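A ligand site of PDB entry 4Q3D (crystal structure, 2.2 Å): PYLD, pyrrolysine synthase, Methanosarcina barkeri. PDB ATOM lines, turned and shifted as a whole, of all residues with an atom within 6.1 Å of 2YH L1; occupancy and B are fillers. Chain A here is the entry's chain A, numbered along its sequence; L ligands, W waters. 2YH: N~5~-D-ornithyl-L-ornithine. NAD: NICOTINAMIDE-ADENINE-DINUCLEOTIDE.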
ATOM      1  N   ALA A   3      -1.499 -16.562 -12.263  1.00  0.00           N
ATOM      2  CA  ALA A   3      -2.584 -16.916 -13.249  1.00  0.00           C
ATOM      3  C   ALA A   3      -3.758 -15.940 -13.128  1.00  0.00           C
ATOM      4  O   ALA A   3      -3.549 -14.749 -12.895  1.00  0.00           O
ATOM      5  CB  ALA A   3      -3.020 -18.361 -13.077  1.00  0.00           C
ATOM      6  N   LEU A   4      -4.986 -16.438 -13.283  1.00  0.00           N
ATOM      7  CA  LEU A   4      -6.176 -15.603 -13.219  1.00  0.00           C
ATOM      8  C   LEU A   4      -6.999 -15.905 -11.971  1.00  0.00           C
ATOM      9  O   LEU A   4      -6.910 -16.995 -11.395  1.00  0.00           O
ATOM     10  CB  LEU A   4      -7.046 -15.807 -14.463  1.00  0.00           C
ATOM     11  CG  LEU A   4      -6.460 -15.218 -15.765  1.00  0.00           C
ATOM     12  CD1 LEU A   4      -7.233 -15.743 -16.961  1.00  0.00           C
ATOM     13  CD2 LEU A   4      -6.470 -13.707 -15.746  1.00  0.00           C
ATOM     14  N   LEU A   5      -7.784 -14.914 -11.557  1.00  0.00           N
ATOM     15  CA  LEU A   5      -8.753 -15.109 -10.495  1.00  0.00           C
ATOM     16  C   LEU A   5      -9.725 -16.230 -10.842  1.00  0.00           C
ATOM     17  O   LEU A   5     -10.085 -16.387 -12.002  1.00  0.00           O
ATOM     18  CB  LEU A   5      -9.543 -13.810 -10.272  1.00  0.00           C
ATOM     19  CG  LEU A   5      -8.791 -12.758  -9.478  1.00  0.00           C
ATOM     20  CD1 LEU A   5      -9.328 -11.377  -9.817  1.00  0.00           C
ATOM     21  CD2 LEU A   5      -8.921 -13.045  -7.985  1.00  0.00           C
ATOM     22  N   VAL A  52     -18.397  -3.569 -17.494  1.00  0.00           N
ATOM     23  CA  VAL A  52     -18.676  -4.277 -18.724  1.00  0.00           C
ATOM     24  C   VAL A  52     -18.017  -5.657 -18.698  1.00  0.00           C
ATOM     25  O   VAL A  52     -16.792  -5.742 -18.684  1.00  0.00           O
ATOM     26  CB  VAL A  52     -18.167  -3.496 -19.962  1.00  0.00           C
ATOM     27  CG1 VAL A  52     -18.506  -4.242 -21.244  1.00  0.00           C
ATOM     28  CG2 VAL A  52     -18.769  -2.106 -19.997  1.00  0.00           C
ATOM     29  N   PRO A  53     -18.823  -6.726 -18.688  1.00  0.00           N
ATOM     30  CA  PRO A  53     -18.233  -8.061 -18.810  1.00  0.00           C
ATOM     31  C   PRO A  53     -17.563  -8.241 -20.170  1.00  0.00           C
ATOM     32  O   PRO A  53     -18.019  -7.683 -21.168  1.00  0.00           O
ATOM     33  CB  PRO A  53     -19.443  -9.010 -18.679  1.00  0.00           C
ATOM     34  CG  PRO A  53     -20.523  -8.185 -18.063  1.00  0.00           C
ATOM     35  CD  PRO A  53     -20.295  -6.795 -18.565  1.00  0.00           C
ATOM     36  N   VAL A  54     -16.472  -8.998 -20.202  1.00  0.00           N
ATOM     37  CA  VAL A  54     -15.677  -9.204 -21.411  1.00  0.00           C
ATOM     38  C   VAL A  54     -15.446 -10.701 -21.627  1.00  0.00           C
ATOM     39  O   VAL A  54     -14.928 -11.398 -20.754  1.00  0.00           O
ATOM     40  CB  VAL A  54     -14.347  -8.424 -21.302  1.00  0.00           C
ATOM     41  CG1 VAL A  54     -13.350  -8.862 -22.373  1.00  0.00           C
ATOM     42  CG2 VAL A  54     -14.604  -6.930 -21.402  1.00  0.00           C
ATOM     43  N   THR A  55     -15.812 -11.191 -22.813  1.00  0.00           N
ATOM     44  CA  THR A  55     -15.707 -12.614 -23.159  1.00  0.00           C
ATOM     45  C   THR A  55     -14.377 -12.976 -23.826  1.00  0.00           C
ATOM     46  O   THR A  55     -14.181 -14.125 -24.223  1.00  0.00           O
ATOM     47  CB  THR A  55     -16.807 -13.018 -24.150  1.00  0.00           C
ATOM     48  OG1 THR A  55     -16.597 -12.338 -25.391  1.00  0.00           O
ATOM     49  CG2 THR A  55     -18.183 -12.670 -23.601  1.00  0.00           C
ATOM     50  N   SER A  56     -13.486 -12.006 -23.954  1.00  0.00           N
ATOM     51  CA  SER A  56     -12.205 -12.199 -24.638  1.00  0.00           C
ATOM     52  C   SER A  56     -11.322 -13.188 -23.892  1.00  0.00           C
ATOM     53  O   SER A  56     -11.389 -13.297 -22.666  1.00  0.00           O
ATOM     54  CB  SER A  56     -11.500 -10.844 -24.814  1.00  0.00           C
ATOM     55  OG  SER A  56     -10.124 -10.921 -24.534  1.00  0.00           O
ATOM     56  N   GLY A  59     -12.386 -15.688 -21.101  1.00  0.00           N
ATOM     57  CA  GLY A  59     -13.793 -15.348 -21.035  1.00  0.00           C
ATOM     58  C   GLY A  59     -14.233 -14.792 -19.695  1.00  0.00           C
ATOM     59  O   GLY A  59     -13.415 -14.419 -18.851  1.00  0.00           O
ATOM     60  N   ILE A  60     -15.546 -14.752 -19.534  1.00  0.00           N
ATOM     61  CA  ILE A  60     -16.172 -14.211 -18.334  1.00  0.00           C
ATOM     62  C   ILE A  60     -15.791 -15.077 -17.134  1.00  0.00           C
ATOM     63  O   ILE A  60     -15.892 -16.307 -17.204  1.00  0.00           O
ATOM     64  CB  ILE A  60     -17.711 -14.124 -18.543  1.00  0.00           C
ATOM     65  CG1 ILE A  60     -18.024 -12.926 -19.444  1.00  0.00           C
ATOM     66  CG2 ILE A  60     -18.445 -13.993 -17.228  1.00  0.00           C
ATOM     67  CD1 ILE A  60     -19.299 -13.067 -20.252  1.00  0.00           C
ATOM     68  N   ILE A  61     -15.311 -14.442 -16.071  1.00  0.00           N
ATOM     69  CA  ILE A  61     -14.940 -15.157 -14.854  1.00  0.00           C
ATOM     70  C   ILE A  61     -16.116 -15.073 -13.870  1.00  0.00           C
ATOM     71  O   ILE A  61     -16.591 -13.980 -13.546  1.00  0.00           O
ATOM     72  CB  ILE A  61     -13.650 -14.608 -14.230  1.00  0.00           C
ATOM     73  CG1 ILE A  61     -12.464 -14.836 -15.165  1.00  0.00           C
ATOM     74  CG2 ILE A  61     -13.350 -15.296 -12.894  1.00  0.00           C
ATOM     75  CD1 ILE A  61     -11.200 -14.120 -14.745  1.00  0.00           C
ATOM     76  N   GLY A  62     -16.577 -16.229 -13.419  1.00  0.00           N
ATOM     77  CA  GLY A  62     -17.671 -16.309 -12.447  1.00  0.00           C
ATOM     78  C   GLY A  62     -17.387 -15.417 -11.265  1.00  0.00           C
ATOM     79  O   GLY A  62     -16.280 -15.414 -10.745  1.00  0.00           O
ATOM     80  N   PHE A  64     -16.885 -12.262 -11.121  1.00  0.00           N
ATOM     81  CA  PHE A  64     -16.015 -11.098 -11.338  1.00  0.00           C
ATOM     82  C   PHE A  64     -16.789  -9.775 -11.419  1.00  0.00           C
ATOM     83  O   PHE A  64     -16.518  -8.857 -10.640  1.00  0.00           O
ATOM     84  CB  PHE A  64     -15.133 -11.291 -12.577  1.00  0.00           C
ATOM     85  CG  PHE A  64     -14.098 -10.224 -12.750  1.00  0.00           C
ATOM     86  CD1 PHE A  64     -12.926 -10.241 -12.003  1.00  0.00           C
ATOM     87  CD2 PHE A  64     -14.291  -9.185 -13.648  1.00  0.00           C
ATOM     88  CE1 PHE A  64     -11.986  -9.241 -12.139  1.00  0.00           C
ATOM     89  CE2 PHE A  64     -13.347  -8.183 -13.794  1.00  0.00           C
ATOM     90  CZ  PHE A  64     -12.189  -8.220 -13.044  1.00  0.00           C
ATOM     91  N   SER A  65     -17.761  -9.682 -12.315  1.00  0.00           N
ATOM     92  CA  SER A  65     -18.567  -8.463 -12.429  1.00  0.00           C
ATOM     93  C   SER A  65     -19.420  -8.244 -11.174  1.00  0.00           C
ATOM     94  O   SER A  65     -19.553  -7.115 -10.691  1.00  0.00           O
ATOM     95  CB  SER A  65     -19.448  -8.492 -13.675  1.00  0.00           C
ATOM     96  OG  SER A  65     -20.298  -9.628 -13.684  1.00  0.00           O
ATOM     97  N   ALA A 104     -12.130  -5.617 -18.005  1.00  0.00           N
ATOM     98  CA  ALA A 104     -10.850  -6.315 -18.007  1.00  0.00           C
ATOM     99  C   ALA A 104     -10.838  -7.430 -19.013  1.00  0.00           C
ATOM    100  O   ALA A 104     -11.830  -8.119 -19.171  1.00  0.00           O
ATOM    101  CB  ALA A 104     -10.563  -6.878 -16.629  1.00  0.00           C
ATOM    102  N   ASP A 105      -9.711  -7.595 -19.706  1.00  0.00           N
ATOM    103  CA  ASP A 105      -9.458  -8.838 -20.439  1.00  0.00           C
ATOM    104  C   ASP A 105      -8.410  -9.628 -19.644  1.00  0.00           C
ATOM    105  O   ASP A 105      -8.226  -9.347 -18.461  1.00  0.00           O
ATOM    106  CB  ASP A 105      -9.164  -8.617 -21.937  1.00  0.00           C
ATOM    107  CG  ASP A 105      -7.901  -7.799 -22.227  1.00  0.00           C
ATOM    108  OD1 ASP A 105      -7.004  -7.645 -21.375  1.00  0.00           O
ATOM    109  OD2 ASP A 105      -7.811  -7.310 -23.368  1.00  0.00           O
ATOM    110  N   ASP A 106      -7.759 -10.615 -20.250  1.00  0.00           N
ATOM    111  CA  ASP A 106      -6.832 -11.465 -19.492  1.00  0.00           C
ATOM    112  C   ASP A 106      -5.494 -10.772 -19.168  1.00  0.00           C
ATOM    113  O   ASP A 106      -4.773 -11.214 -18.275  1.00  0.00           O
ATOM    114  CB  ASP A 106      -6.576 -12.779 -20.227  1.00  0.00           C
ATOM    115  CG  ASP A 106      -7.804 -13.673 -20.298  1.00  0.00           C
ATOM    116  OD1 ASP A 106      -8.826 -13.370 -19.646  1.00  0.00           O
ATOM    117  OD2 ASP A 106      -7.751 -14.685 -21.028  1.00  0.00           O
ATOM    118  N   ARG A 107      -5.180  -9.696 -19.887  1.00  0.00           N
ATOM    119  CA  ARG A 107      -3.915  -8.979 -19.707  1.00  0.00           C
ATOM    120  C   ARG A 107      -4.068  -7.558 -19.107  1.00  0.00           C
ATOM    121  O   ARG A 107      -3.117  -7.039 -18.531  1.00  0.00           O
ATOM    122  CB  ARG A 107      -3.137  -8.974 -21.043  1.00  0.00           C
ATOM    123  CG  ARG A 107      -2.594  -7.635 -21.545  1.00  0.00           C
ATOM    124  CD  ARG A 107      -1.169  -7.735 -22.068  1.00  0.00           C
ATOM    125  NE  ARG A 107      -0.198  -7.495 -21.007  1.00  0.00           N
ATOM    126  CZ  ARG A 107       1.109  -7.746 -21.094  1.00  0.00           C
ATOM    127  NH1 ARG A 107       1.642  -8.252 -22.202  1.00  0.00           N
ATOM    128  NH2 ARG A 107       1.894  -7.487 -20.045  1.00  0.00           N
ATOM    129  N   THR A 108      -5.254  -6.961 -19.220  1.00  0.00           N
ATOM    130  CA  THR A 108      -5.468  -5.579 -18.760  1.00  0.00           C
ATOM    131  C   THR A 108      -6.822  -5.392 -18.083  1.00  0.00           C
ATOM    132  O   THR A 108      -7.873  -5.696 -18.643  1.00  0.00           O
ATOM    133  CB  THR A 108      -5.385  -4.563 -19.927  1.00  0.00           C
ATOM    134  OG1 THR A 108      -4.089  -4.641 -20.528  1.00  0.00           O
ATOM    135  CG2 THR A 108      -5.598  -3.138 -19.426  1.00  0.00           C
ATOM    136  N   PHE A 109      -6.771  -4.858 -16.867  1.00  0.00           N
ATOM    137  CA  PHE A 109      -7.946  -4.432 -16.139  1.00  0.00           C
ATOM    138  C   PHE A 109      -7.806  -2.933 -15.945  1.00  0.00           C
ATOM    139  O   PHE A 109      -6.824  -2.464 -15.378  1.00  0.00           O
ATOM    140  CB  PHE A 109      -8.049  -5.206 -14.810  1.00  0.00           C
ATOM    141  CG  PHE A 109      -9.151  -4.744 -13.884  1.00  0.00           C
ATOM    142  CD1 PHE A 109     -10.310  -4.130 -14.364  1.00  0.00           C
ATOM    143  CD2 PHE A 109      -9.037  -4.962 -12.512  1.00  0.00           C
ATOM    144  CE1 PHE A 109     -11.303  -3.721 -13.494  1.00  0.00           C
ATOM    145  CE2 PHE A 109     -10.039  -4.552 -11.645  1.00  0.00           C
ATOM    146  CZ  PHE A 109     -11.172  -3.927 -12.135  1.00  0.00           C
ATOM    147  N   ASN A 121      -4.539   1.586 -14.776  1.00  0.00           N
ATOM    148  CA  ASN A 121      -4.287   0.159 -14.937  1.00  0.00           C
ATOM    149  C   ASN A 121      -4.213  -0.489 -13.559  1.00  0.00           C
ATOM    150  O   ASN A 121      -3.558   0.032 -12.659  1.00  0.00           O
ATOM    151  CB  ASN A 121      -2.990  -0.077 -15.710  1.00  0.00           C
ATOM    152  CG  ASN A 121      -2.773  -1.536 -16.054  1.00  0.00           C
ATOM    153  OD1 ASN A 121      -2.797  -2.408 -15.183  1.00  0.00           O
ATOM    154  ND2 ASN A 121      -2.536  -1.819 -17.339  1.00  0.00           N
ATOM    155  N   ASN A 122      -4.864  -1.626 -13.405  1.00  0.00           N
ATOM    156  CA  ASN A 122      -4.962  -2.318 -12.124  1.00  0.00           C
ATOM    157  C   ASN A 122      -3.626  -2.751 -11.517  1.00  0.00           C
ATOM    158  O   ASN A 122      -3.495  -2.824 -10.295  1.00  0.00           O
ATOM    159  CB  ASN A 122      -5.846  -3.559 -12.308  1.00  0.00           C
ATOM    160  CG  ASN A 122      -5.868  -4.445 -11.091  1.00  0.00           C
ATOM    161  OD1 ASN A 122      -5.258  -5.508 -11.096  1.00  0.00           O
ATOM    162  ND2 ASN A 122      -6.561  -4.014 -10.037  1.00  0.00           N
ATOM    163  N   GLN A 123      -2.625  -3.031 -12.369  1.00  0.00           N
ATOM    164  CA  GLN A 123      -1.342  -3.539 -11.874  1.00  0.00           C
ATOM    165  C   GLN A 123      -0.551  -2.509 -11.081  1.00  0.00           C
ATOM    166  O   GLN A 123      -0.182  -2.761  -9.924  1.00  0.00           O
ATOM    167  CB  GLN A 123      -0.502  -4.123 -13.001  1.00  0.00           C
ATOM    168  CG  GLN A 123      -0.896  -5.542 -13.384  1.00  0.00           C
ATOM    169  CD  GLN A 123      -0.680  -5.837 -14.854  1.00  0.00           C
ATOM    170  OE1 GLN A 123      -0.513  -4.921 -15.661  1.00  0.00           O
ATOM    171  NE2 GLN A 123      -0.683  -7.101 -15.209  1.00  0.00           N
HETATM  172  O3  2YH L   1      -7.960 -10.383 -13.745  1.00  0.00           O
HETATM  173  C6  2YH L   1      -7.683 -10.149 -14.921  1.00  0.00           C
HETATM  174  C7  2YH L   1      -6.364  -9.474 -15.174  1.00  0.00           C
HETATM  175  N3  2YH L   1      -6.140  -8.861 -16.533  1.00  0.00           N
HETATM  176  C8  2YH L   1      -5.235 -10.463 -14.847  1.00  0.00           C
HETATM  177  C9  2YH L   1      -4.172  -9.788 -13.967  1.00  0.00           C
HETATM  178  C10 2YH L   1      -3.766  -8.387 -14.455  1.00  0.00           C
HETATM  179  N2  2YH L   1      -4.381  -7.291 -13.650  1.00  0.00           N
HETATM  180  N1  2YH L   1      -8.546 -10.506 -15.931  1.00  0.00           N
HETATM  181  C5  2YH L   1      -9.941 -10.628 -15.475  1.00  0.00           C
HETATM  182  C4  2YH L   1     -10.841 -10.988 -16.653  1.00  0.00           C
HETATM  183  C3  2YH L   1     -12.302 -10.606 -16.391  1.00  0.00           C
HETATM  184  C2  2YH L   1     -13.259 -11.346 -17.319  1.00  0.00           C
HETATM  185  N4  2YH L   1     -12.983 -11.014 -18.759  1.00  0.00           N
HETATM  186  C1  2YH L   1     -14.664 -10.998 -16.956  1.00  0.00           C
HETATM  187  O2  2YH L   1     -15.299 -11.687 -16.173  1.00  0.00           O
HETATM  188  O1  2YH L   1     -15.252  -9.922 -17.485  1.00  0.00           O
HETATM  189  PA  NAD L   2       4.268 -10.804 -12.440  1.00  0.00           P
HETATM  190  O1A NAD L   2       4.392 -12.169 -13.061  1.00  0.00           O
HETATM  191  O2A NAD L   2       4.310  -9.565 -13.306  1.00  0.00           O
HETATM  192  O5B NAD L   2       5.407 -10.685 -11.318  1.00  0.00           O
HETATM  193  C5B NAD L   2       5.484 -11.635 -10.250  1.00  0.00           C
HETATM  194  C4B NAD L   2       6.944 -11.758  -9.861  1.00  0.00           C
HETATM  195  O4B NAD L   2       7.112 -12.604  -8.716  1.00  0.00           O
HETATM  196  C3B NAD L   2       7.781 -12.363 -10.983  1.00  0.00           C
HETATM  197  O3B NAD L   2       8.738 -11.396 -11.446  1.00  0.00           O
HETATM  198  C2B NAD L   2       8.468 -13.566 -10.354  1.00  0.00           C
HETATM  199  O2B NAD L   2       9.833 -13.746 -10.732  1.00  0.00           O
HETATM  200  C1B NAD L   2       8.370 -13.256  -8.881  1.00  0.00           C
HETATM  201  N9A NAD L   2       8.538 -14.460  -8.026  1.00  0.00           N
HETATM  202  C8A NAD L   2       8.009 -15.687  -8.182  1.00  0.00           C
HETATM  203  N7A NAD L   2       8.414 -16.510  -7.182  1.00  0.00           N
HETATM  204  C5A NAD L   2       9.226 -15.812  -6.371  1.00  0.00           C
HETATM  205  C6A NAD L   2      10.006 -16.045  -5.131  1.00  0.00           C
HETATM  206  N6A NAD L   2      10.001 -17.257  -4.539  1.00  0.00           N
HETATM  207  N1A NAD L   2      10.716 -15.022  -4.620  1.00  0.00           N
HETATM  208  C2A NAD L   2      10.737 -13.804  -5.193  1.00  0.00           C
HETATM  209  N3A NAD L   2      10.061 -13.518  -6.318  1.00  0.00           N
HETATM  210  C4A NAD L   2       9.303 -14.454  -6.938  1.00  0.00           C
HETATM  211  O3  NAD L   2       2.920 -10.802 -11.570  1.00  0.00           O
HETATM  212  PN  NAD L   2       2.122  -9.455 -11.187  1.00  0.00           P
HETATM  213  O1N NAD L   2       1.205  -9.115 -12.339  1.00  0.00           O
HETATM  214  O2N NAD L   2       3.097  -8.439 -10.643  1.00  0.00           O
HETATM  215  O5D NAD L   2       1.175  -9.969  -9.986  1.00  0.00           O
HETATM  216  C5D NAD L   2       1.676 -10.768  -8.922  1.00  0.00           C
HETATM  217  C4D NAD L   2       0.510 -11.356  -8.146  1.00  0.00           C
HETATM  218  O4D NAD L   2      -0.390 -10.324  -7.757  1.00  0.00           O
HETATM  219  C3D NAD L   2      -0.305 -12.362  -8.954  1.00  0.00           C
HETATM  220  O3D NAD L   2      -0.614 -13.498  -8.147  1.00  0.00           O
HETATM  221  C2D NAD L   2      -1.587 -11.631  -9.294  1.00  0.00           C
HETATM  222  O2D NAD L   2      -2.701 -12.513  -9.440  1.00  0.00           O
HETATM  223  C1D NAD L   2      -1.728 -10.746  -8.058  1.00  0.00           C
HETATM  224  N1N NAD L   2      -2.605  -9.571  -8.197  1.00  0.00           N
HETATM  225  C2N NAD L   2      -3.469  -9.345  -7.206  1.00  0.00           C
HETATM  226  C3N NAD L   2      -4.327  -8.250  -7.213  1.00  0.00           C
HETATM  227  C7N NAD L   2      -5.296  -8.012  -6.075  1.00  0.00           C
HETATM  228  O7N NAD L   2      -6.177  -7.183  -6.221  1.00  0.00           O
HETATM  229  N7N NAD L   2      -5.197  -8.694  -4.923  1.00  0.00           N
HETATM  230  C4N NAD L   2      -4.268  -7.373  -8.298  1.00  0.00           C
HETATM  231  C5N NAD L   2      -3.350  -7.623  -9.328  1.00  0.00           C
HETATM  232  C6N NAD L   2      -2.516  -8.731  -9.257  1.00  0.00           C
HETATM  233  O   HOH W   1      -1.425  -8.925 -12.660  1.00  0.00           O
HETATM  234  O   HOH W   2      -6.389 -12.148 -11.881  1.00  0.00           O
HETATM  235  O   HOH W   3     -16.789  -7.564 -15.502  1.00  0.00           O
HETATM  236  O   HOH W   4     -14.510  -7.091 -17.631  1.00  0.00           O
HETATM  237  O   HOH W   5      -5.026  -9.808 -10.844  1.00  0.00           O
HETATM  238  O   HOH W   6     -10.922 -11.787 -20.341  1.00  0.00           O
HETATM  239  O   HOH W   7     -17.816 -10.374 -15.744  1.00  0.00           O
HETATM  240  O   HOH W   8      -4.027  -4.607 -15.803  1.00  0.00           O
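The backbone carbonyl oxygen (O) of Ala 104 is in hydrogen-bond range of a nitrogen (N4) of 2YH L1, at 3.1 Å. A nitrogen (N4) of 2YH L1 is in hydrogen-bond range of the backbone carbonyl oxygen (O) of Gly 59, 3.4 Å away. O of Val 54 lies within hydrogen-bond range of N4 of 2YH L1 (2.8 Å). A nitrogen (N1) of 2YH L1 is in hydrogen-bond range of the backbone carbonyl oxygen (O) of Asp 105, 2.8 Å away. The backbone NH (N) of Thr 108 sits close to a nitrogen (N3) of 2YH L1 (3.4 Å). N of Val 54 is in hydrogen-bond range of O1 of 2YH L1 (3.1 Å). O of Asp 106 sits at hydrogen-bond distance from N3 of 2YH L1 (3.2 Å). OD1 of Asn 122 sits at hydrogen-bond distance from N2 of 2YH L1 (3.2 Å). N of Ile 61 lies within hydrogen-bond range of O2 of 2YH L1, 2.8 Å away.
The backbone NH (N) of Asn 122 lies within hydrogen-bond range of the backbone carbonyl oxygen (O) of Phe 109 (2.9 Å). The backbone NH of Thr 108 sits at hydrogen-bond distance from the side-chain carboxylate of Asp 105. The side-chain carboxylate (OD1) of Asp 105 lies within hydrogen-bond range of the backbone NH (N) of Arg 107. The side-chain amide oxygen (OD1) of Asn 121 sits at hydrogen-bond distance from the backbone NH (N) of Gln 123 (2.9 Å).
Leu 4 touches 2YH L1. CA of Pro 53 touches O1 of 2YH L1 (3.8 Å). Ile 60 touches 2YH L1. Phe 64 touches 2YH L1 (CB to O2, 3.6 Å). Arg 107 touches 2YH L1. Gln 123 touches 2YH L1 (NE2 to C10, 3.4 Å). Of the 23 residues printed, 14 come within 4 Å of 2YH L1.
Water W6 lies within hydrogen-bond range of N4 of 2YH L1 (2.7 Å), OD1 of Asp 106 (2.7 Å) and O of Ser 56 (2.8 Å). Water W7 lies within hydrogen-bond range of an oxygen (O2) of 2YH L1 (2.9 Å) and the side-chain hydroxyl (OG) of Ser 65 (3.3 Å). Water W4 lies within hydrogen-bond range of the backbone NH of Ala 104 (2.8 Å), the backbone carbonyl oxygen of Val 52 (2.9 Å) and an oxygen (O1) of 2YH L1 (2.9 Å). Water W1 bridges O1N of NAD L2 and NE2 of Gln 123. Water W2 bridges O3 of 2YH L1 and N of Leu 5. Water W8 lies within hydrogen-bond range of OD1 of Asn 121 (2.6 Å), N of Phe 109 (3.0 Å) and N2 of 2YH L1 (3.5 Å).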
